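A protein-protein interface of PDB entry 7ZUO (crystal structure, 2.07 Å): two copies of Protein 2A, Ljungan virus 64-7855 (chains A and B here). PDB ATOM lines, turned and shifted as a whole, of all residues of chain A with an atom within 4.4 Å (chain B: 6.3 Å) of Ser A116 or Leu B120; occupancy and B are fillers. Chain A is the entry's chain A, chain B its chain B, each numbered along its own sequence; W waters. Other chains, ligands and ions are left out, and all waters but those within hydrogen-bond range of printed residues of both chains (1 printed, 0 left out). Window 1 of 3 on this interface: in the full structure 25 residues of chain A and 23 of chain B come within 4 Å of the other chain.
O of Leu A112 lies within hydrogen-bond range of OG of Ser A116 (2.6 Å).
Among the printed residues, merely in contact across the chains: Val A75 with Tyr B70 (3.4 Å), Gly A76 with Leu B123 (3.5 Å), Ser A116 with Leu B120 (3.6 Å), Leu A119 with Leu B119 (3.6 Å), Gly A76 with Ala B124 (3.6 Å), Ser A116 with Leu B123 (3.6 Å), Val A75 with Leu B120 (3.8 Å), Leu A115 with Leu B123 (3.8 Å), Leu A120 with Ser B116 (3.8 Å), Val A75 with Leu B123 (3.8 Å), Leu A120 with Leu B119 (3.9 Å), Leu A119 with Leu B123 (3.9 Å), Leu A112 with Leu B123 (3.9 Å) and Leu A119 with Leu B122 (3.995 Å).
Ser A116 touches two residues of chain B. Printed residues of chain A within 4 Å of Leu B120: Val A75 (3.8 Å) and Ser A116 (3.6 Å). Printed residues of chain A within 4 Å of Ser B116: Leu A120. Printed residues of chain A within 4 Å of Leu B122: Leu A119.
Printed residues of chain B that touch a printed residue of chain A: Tyr B70, Ser B116, Leu B119, Leu B120, Leu B122, Leu B123 and Ala B124. Hydrophobic or aromatic side chains of chain B within 4 Å of the printed part of chain A: Tyr B70, Leu B119, Leu B120, Leu B122, Leu B123 and Ala B124. Among the printed residues, no Asp or Glu carboxylate lies within 4 Å of a Lys or Arg side-chain nitrogen of the other chain.
Ser A116 touches Leu B120, and with the chains exchanged Leu A120 touches Ser B116. Leu A119 touches its own counterpart, Leu B119. Leu A120 touches Leu B119, but with the chains exchanged Leu A119 does not touch Leu B120 (4.3 Å). Positions printed for both chains: 70, 115, 116, 117, 118, 119 and 120. Of the 14 pairs that touch across the chains among the printed residues, 3 have their exchanged pair printed and touching as well.
Water W1 lies within hydrogen-bond range of O of Gly A76 (2.8 Å) and O of Leu B120 (3.1 Å).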
ATOM      1  N   TYR A  70     -18.290  -0.962 -11.992  1.00  0.00           N
ATOM      2  CA  TYR A  70     -18.168   0.488 -12.072  1.00  0.00           C
ATOM      3  C   TYR A  70     -16.772   0.973 -12.469  1.00  0.00           C
ATOM      4  O   TYR A  70     -16.595   2.175 -12.665  1.00  0.00           O
ATOM      5  CB  TYR A  70     -18.620   1.115 -10.744  1.00  0.00           C
ATOM      6  CG  TYR A  70     -20.045   0.766 -10.371  1.00  0.00           C
ATOM      7  CD1 TYR A  70     -21.060   0.776 -11.318  1.00  0.00           C
ATOM      8  CD2 TYR A  70     -20.380   0.405  -9.075  1.00  0.00           C
ATOM      9  CE1 TYR A  70     -22.361   0.421 -10.984  1.00  0.00           C
ATOM     10  CE2 TYR A  70     -21.686   0.080  -8.717  1.00  0.00           C
ATOM     11  CZ  TYR A  70     -22.678   0.089  -9.672  1.00  0.00           C
ATOM     12  OH  TYR A  70     -23.983  -0.232  -9.335  1.00  0.00           O
ATOM     13  N   VAL A  75     -17.718   1.795 -18.598  1.00  0.00           N
ATOM     14  CA  VAL A  75     -18.033   2.960 -17.778  1.00  0.00           C
ATOM     15  C   VAL A  75     -16.986   4.056 -17.962  1.00  0.00           C
ATOM     16  O   VAL A  75     -16.073   4.203 -17.163  1.00  0.00           O
ATOM     17  CB  VAL A  75     -18.213   2.549 -16.307  1.00  0.00           C
ATOM     18  CG1 VAL A  75     -18.432   3.737 -15.397  1.00  0.00           C
ATOM     19  CG2 VAL A  75     -19.370   1.562 -16.186  1.00  0.00           C
ATOM     20  N   GLY A  76     -17.155   4.874 -18.997  1.00  0.00           N
ATOM     21  CA  GLY A  76     -16.277   6.019 -19.194  1.00  0.00           C
ATOM     22  C   GLY A  76     -16.456   7.066 -18.095  1.00  0.00           C
ATOM     23  O   GLY A  76     -17.531   7.193 -17.516  1.00  0.00           O
ATOM     24  N   LEU A 112     -15.432   6.180  -8.241  1.00  0.00           N
ATOM     25  CA  LEU A 112     -16.285   5.688  -9.312  1.00  0.00           C
ATOM     26  C   LEU A 112     -17.405   4.827  -8.726  1.00  0.00           C
ATOM     27  O   LEU A 112     -18.514   4.795  -9.239  1.00  0.00           O
ATOM     28  CB  LEU A 112     -15.458   4.877 -10.311  1.00  0.00           C
ATOM     29  CG  LEU A 112     -14.643   5.684 -11.322  1.00  0.00           C
ATOM     30  CD1 LEU A 112     -13.730   4.777 -12.132  1.00  0.00           C
ATOM     31  CD2 LEU A 112     -15.557   6.448 -12.245  1.00  0.00           C
ATOM     32  N   ILE A 113     -17.099   4.049  -7.696  1.00  0.00           N
ATOM     33  CA  ILE A 113     -18.143   3.238  -7.100  1.00  0.00           C
ATOM     34  C   ILE A 113     -19.226   4.144  -6.505  1.00  0.00           C
ATOM     35  O   ILE A 113     -20.408   3.933  -6.762  1.00  0.00           O
ATOM     36  CB  ILE A 113     -17.568   2.262  -6.057  1.00  0.00           C
ATOM     37  CG1 ILE A 113     -16.687   1.202  -6.726  1.00  0.00           C
ATOM     38  CG2 ILE A 113     -18.705   1.638  -5.243  1.00  0.00           C
ATOM     39  CD1 ILE A 113     -15.834   0.439  -5.734  1.00  0.00           C
ATOM     40  N   LEU A 114     -18.814   5.161  -5.744  1.00  0.00           N
ATOM     41  CA  LEU A 114     -19.769   5.978  -5.019  1.00  0.00           C
ATOM     42  C   LEU A 114     -20.622   6.801  -5.987  1.00  0.00           C
ATOM     43  O   LEU A 114     -21.820   6.946  -5.768  1.00  0.00           O
ATOM     44  CB  LEU A 114     -19.042   6.876  -4.007  1.00  0.00           C
ATOM     45  CG  LEU A 114     -18.310   6.129  -2.897  1.00  0.00           C
ATOM     46  CD1 LEU A 114     -17.613   7.091  -1.953  1.00  0.00           C
ATOM     47  CD2 LEU A 114     -19.274   5.245  -2.141  1.00  0.00           C
ATOM     48  N   LEU A 115     -20.030   7.339  -7.057  1.00  0.00           N
ATOM     49  CA  LEU A 115     -20.803   8.183  -7.958  1.00  0.00           C
ATOM     50  C   LEU A 115     -21.733   7.301  -8.786  1.00  0.00           C
ATOM     51  O   LEU A 115     -22.868   7.689  -9.053  1.00  0.00           O
ATOM     52  CB  LEU A 115     -19.902   8.982  -8.902  1.00  0.00           C
ATOM     53  CG  LEU A 115     -19.092  10.140  -8.312  1.00  0.00           C
ATOM     54  CD1 LEU A 115     -18.240  10.795  -9.401  1.00  0.00           C
ATOM     55  CD2 LEU A 115     -20.002  11.190  -7.670  1.00  0.00           C
ATOM     56  N   SER A 116     -21.229   6.137  -9.206  1.00  0.00           N
ATOM     57  CA  SER A 116     -22.014   5.200  -9.989  1.00  0.00           C
ATOM     58  C   SER A 116     -23.252   4.744  -9.203  1.00  0.00           C
ATOM     59  O   SER A 116     -24.360   4.699  -9.742  1.00  0.00           O
ATOM     60  CB  SER A 116     -21.173   4.017 -10.449  1.00  0.00           C
ATOM     61  OG  SER A 116     -20.095   4.422 -11.294  1.00  0.00           O
ATOM     62  N   ALA A 117     -23.056   4.398  -7.926  1.00  0.00           N
ATOM     63  CA  ALA A 117     -24.150   3.956  -7.075  1.00  0.00           C
ATOM     64  C   ALA A 117     -25.198   5.072  -6.968  1.00  0.00           C
ATOM     65  O   ALA A 117     -26.392   4.827  -7.116  1.00  0.00           O
ATOM     66  CB  ALA A 117     -23.622   3.515  -5.737  1.00  0.00           C
ATOM     67  N   SER A 118     -24.742   6.311  -6.726  1.00  0.00           N
ATOM     68  CA  SER A 118     -25.639   7.442  -6.588  1.00  0.00           C
ATOM     69  C   SER A 118     -26.451   7.622  -7.865  1.00  0.00           C
ATOM     70  O   SER A 118     -27.681   7.789  -7.827  1.00  0.00           O
ATOM     71  CB  SER A 118     -24.850   8.663  -6.242  1.00  0.00           C
ATOM     72  OG  SER A 118     -25.701   9.707  -5.866  1.00  0.00           O
ATOM     73  N   LEU A 119     -25.756   7.564  -9.014  1.00  0.00           N
ATOM     74  CA  LEU A 119     -26.449   7.698 -10.276  1.00  0.00           C
ATOM     75  C   LEU A 119     -27.479   6.581 -10.448  1.00  0.00           C
ATOM     76  O   LEU A 119     -28.616   6.846 -10.859  1.00  0.00           O
ATOM     77  CB  LEU A 119     -25.444   7.700 -11.427  1.00  0.00           C
ATOM     78  CG  LEU A 119     -24.660   8.986 -11.598  1.00  0.00           C
ATOM     79  CD1 LEU A 119     -23.551   8.791 -12.612  1.00  0.00           C
ATOM     80  CD2 LEU A 119     -25.581  10.125 -12.034  1.00  0.00           C
ATOM     81  N   LEU A 120     -27.104   5.323 -10.157  1.00  0.00           N
ATOM     82  CA  LEU A 120     -28.037   4.232 -10.401  1.00  0.00           C
ATOM     83  C   LEU A 120     -29.148   4.172  -9.332  1.00  0.00           C
ATOM     84  O   LEU A 120     -30.180   3.571  -9.593  1.00  0.00           O
ATOM     85  CB  LEU A 120     -27.243   2.928 -10.543  1.00  0.00           C
ATOM     86  CG  LEU A 120     -26.370   2.855 -11.796  1.00  0.00           C
ATOM     87  CD1 LEU A 120     -25.683   1.518 -11.923  1.00  0.00           C
ATOM     88  CD2 LEU A 120     -27.181   3.106 -13.037  1.00  0.00           C
ATOM     89  N   TYR B  19     -27.900   5.149 -25.003  1.00  0.00           N
ATOM     90  CA  TYR B  19     -27.351   3.886 -25.451  1.00  0.00           C
ATOM     91  C   TYR B  19     -28.415   3.046 -26.143  1.00  0.00           C
ATOM     92  O   TYR B  19     -29.618   3.134 -25.839  1.00  0.00           O
ATOM     93  CB  TYR B  19     -26.732   3.118 -24.283  1.00  0.00           C
ATOM     94  CG  TYR B  19     -25.355   3.570 -23.885  1.00  0.00           C
ATOM     95  CD1 TYR B  19     -25.165   4.670 -23.073  1.00  0.00           C
ATOM     96  CD2 TYR B  19     -24.226   2.922 -24.370  1.00  0.00           C
ATOM     97  CE1 TYR B  19     -23.891   5.093 -22.727  1.00  0.00           C
ATOM     98  CE2 TYR B  19     -22.943   3.322 -24.030  1.00  0.00           C
ATOM     99  CZ  TYR B  19     -22.783   4.398 -23.181  1.00  0.00           C
ATOM    100  OH  TYR B  19     -21.550   4.827 -22.811  1.00  0.00           O
ATOM    101  N   TYR B  70     -25.061  -5.514 -14.811  1.00  0.00           N
ATOM    102  CA  TYR B  70     -26.086  -4.477 -14.666  1.00  0.00           C
ATOM    103  C   TYR B  70     -27.440  -5.053 -14.239  1.00  0.00           C
ATOM    104  O   TYR B  70     -28.323  -4.283 -13.855  1.00  0.00           O
ATOM    105  CB  TYR B  70     -26.106  -3.565 -15.907  1.00  0.00           C
ATOM    106  CG  TYR B  70     -24.758  -2.913 -16.028  1.00  0.00           C
ATOM    107  CD1 TYR B  70     -24.254  -2.133 -15.001  1.00  0.00           C
ATOM    108  CD2 TYR B  70     -23.918  -3.201 -17.087  1.00  0.00           C
ATOM    109  CE1 TYR B  70     -22.950  -1.667 -15.012  1.00  0.00           C
ATOM    110  CE2 TYR B  70     -22.624  -2.704 -17.133  1.00  0.00           C
ATOM    111  CZ  TYR B  70     -22.124  -1.953 -16.089  1.00  0.00           C
ATOM    112  OH  TYR B  70     -20.828  -1.487 -16.172  1.00  0.00           O
ATOM    113  N   LEU B 115     -30.467   1.444 -19.459  1.00  0.00           N
ATOM    114  CA  LEU B 115     -30.695   2.456 -18.447  1.00  0.00           C
ATOM    115  C   LEU B 115     -29.385   2.705 -17.701  1.00  0.00           C
ATOM    116  O   LEU B 115     -29.055   3.854 -17.382  1.00  0.00           O
ATOM    117  CB  LEU B 115     -31.777   1.993 -17.465  1.00  0.00           C
ATOM    118  CG  LEU B 115     -33.223   1.955 -17.942  1.00  0.00           C
ATOM    119  CD1 LEU B 115     -34.103   1.303 -16.870  1.00  0.00           C
ATOM    120  CD2 LEU B 115     -33.745   3.344 -18.268  1.00  0.00           C
ATOM    121  N   SER B 116     -28.692   1.616 -17.348  1.00  0.00           N
ATOM    122  CA  SER B 116     -27.484   1.712 -16.547  1.00  0.00           C
ATOM    123  C   SER B 116     -26.390   2.469 -17.292  1.00  0.00           C
ATOM    124  O   SER B 116     -25.764   3.370 -16.736  1.00  0.00           O
ATOM    125  CB  SER B 116     -27.011   0.362 -16.075  1.00  0.00           C
ATOM    126  OG  SER B 116     -28.014  -0.253 -15.271  1.00  0.00           O
ATOM    127  N   ALA B 117     -26.162   2.101 -18.554  1.00  0.00           N
ATOM    128  CA  ALA B 117     -25.160   2.762 -19.368  1.00  0.00           C
ATOM    129  C   ALA B 117     -25.518   4.237 -19.576  1.00  0.00           C
ATOM    130  O   ALA B 117     -24.668   5.123 -19.465  1.00  0.00           O
ATOM    131  CB  ALA B 117     -25.033   2.022 -20.681  1.00  0.00           C
ATOM    132  N   SER B 118     -26.796   4.503 -19.864  1.00  0.00           N
ATOM    133  CA  SER B 118     -27.243   5.872 -20.077  1.00  0.00           C
ATOM    134  C   SER B 118     -27.048   6.737 -18.819  1.00  0.00           C
ATOM    135  O   SER B 118     -26.623   7.893 -18.915  1.00  0.00           O
ATOM    136  CB  SER B 118     -28.694   5.895 -20.567  1.00  0.00           C
ATOM    137  OG  SER B 118     -28.855   5.191 -21.787  1.00  0.00           O
ATOM    138  N   LEU B 119     -27.375   6.211 -17.632  1.00  0.00           N
ATOM    139  CA  LEU B 119     -27.162   6.940 -16.386  1.00  0.00           C
ATOM    140  C   LEU B 119     -25.673   7.135 -16.099  1.00  0.00           C
ATOM    141  O   LEU B 119     -25.240   8.239 -15.750  1.00  0.00           O
ATOM    142  CB  LEU B 119     -27.853   6.218 -15.213  1.00  0.00           C
ATOM    143  CG  LEU B 119     -29.365   6.476 -15.117  1.00  0.00           C
ATOM    144  CD1 LEU B 119     -30.037   5.550 -14.130  1.00  0.00           C
ATOM    145  CD2 LEU B 119     -29.655   7.924 -14.734  1.00  0.00           C
ATOM    146  N   LEU B 120     -24.889   6.074 -16.267  1.00  0.00           N
ATOM    147  CA  LEU B 120     -23.468   6.149 -15.972  1.00  0.00           C
ATOM    148  C   LEU B 120     -22.726   7.039 -16.960  1.00  0.00           C
ATOM    149  O   LEU B 120     -21.644   7.504 -16.640  1.00  0.00           O
ATOM    150  CB  LEU B 120     -22.873   4.745 -15.943  1.00  0.00           C
ATOM    151  CG  LEU B 120     -23.388   3.879 -14.802  1.00  0.00           C
ATOM    152  CD1 LEU B 120     -22.762   2.511 -14.892  1.00  0.00           C
ATOM    153  CD2 LEU B 120     -23.112   4.507 -13.448  1.00  0.00           C
ATOM    154  N   SER B 121     -23.308   7.313 -18.131  1.00  0.00           N
ATOM    155  CA  SER B 121     -22.700   8.234 -19.081  1.00  0.00           C
ATOM    156  C   SER B 121     -22.539   9.637 -18.494  1.00  0.00           C
ATOM    157  O   SER B 121     -21.785  10.423 -19.044  1.00  0.00           O
ATOM    158  CB  SER B 121     -23.474   8.312 -20.363  1.00  0.00           C
ATOM    159  OG  SER B 121     -24.657   9.066 -20.191  1.00  0.00           O
ATOM    160  N   LEU B 122     -23.266   9.982 -17.419  1.00  0.00           N
ATOM    161  CA  LEU B 122     -23.080  11.281 -16.794  1.00  0.00           C
ATOM    162  C   LEU B 122     -21.671  11.452 -16.211  1.00  0.00           C
ATOM    163  O   LEU B 122     -21.250  12.581 -15.997  1.00  0.00           O
ATOM    164  CB  LEU B 122     -24.155  11.481 -15.724  1.00  0.00           C
ATOM    165  CG  LEU B 122     -25.418  12.167 -16.236  1.00  0.00           C
ATOM    166  CD1 LEU B 122     -26.240  11.254 -17.128  1.00  0.00           C
ATOM    167  CD2 LEU B 122     -26.243  12.642 -15.065  1.00  0.00           C
ATOM    168  N   LEU B 123     -20.926  10.355 -15.957  1.00  0.00           N
ATOM    169  CA  LEU B 123     -19.550  10.462 -15.476  1.00  0.00           C
ATOM    170  C   LEU B 123     -18.641  10.984 -16.591  1.00  0.00           C
ATOM    171  O   LEU B 123     -17.565  11.509 -16.344  1.00  0.00           O
ATOM    172  CB  LEU B 123     -19.040   9.082 -15.045  1.00  0.00           C
ATOM    173  CG  LEU B 123     -19.786   8.412 -13.902  1.00  0.00           C
ATOM    174  CD1 LEU B 123     -19.170   7.056 -13.622  1.00  0.00           C
ATOM    175  CD2 LEU B 123     -19.724   9.274 -12.661  1.00  0.00           C
ATOM    176  N   ALA B 124     -19.087  10.759 -17.820  1.00  0.00           N
ATOM    177  CA  ALA B 124     -18.265  10.884 -19.003  1.00  0.00           C
ATOM    178  C   ALA B 124     -18.527  12.213 -19.701  1.00  0.00           C
ATOM    179  O   ALA B 124     -17.581  12.765 -20.237  1.00  0.00           O
ATOM    180  CB  ALA B 124     -18.530   9.715 -19.926  1.00  0.00           C
HETATM  181  O   HOH W   1     -19.823   6.246 -18.749  1.00  0.00           O
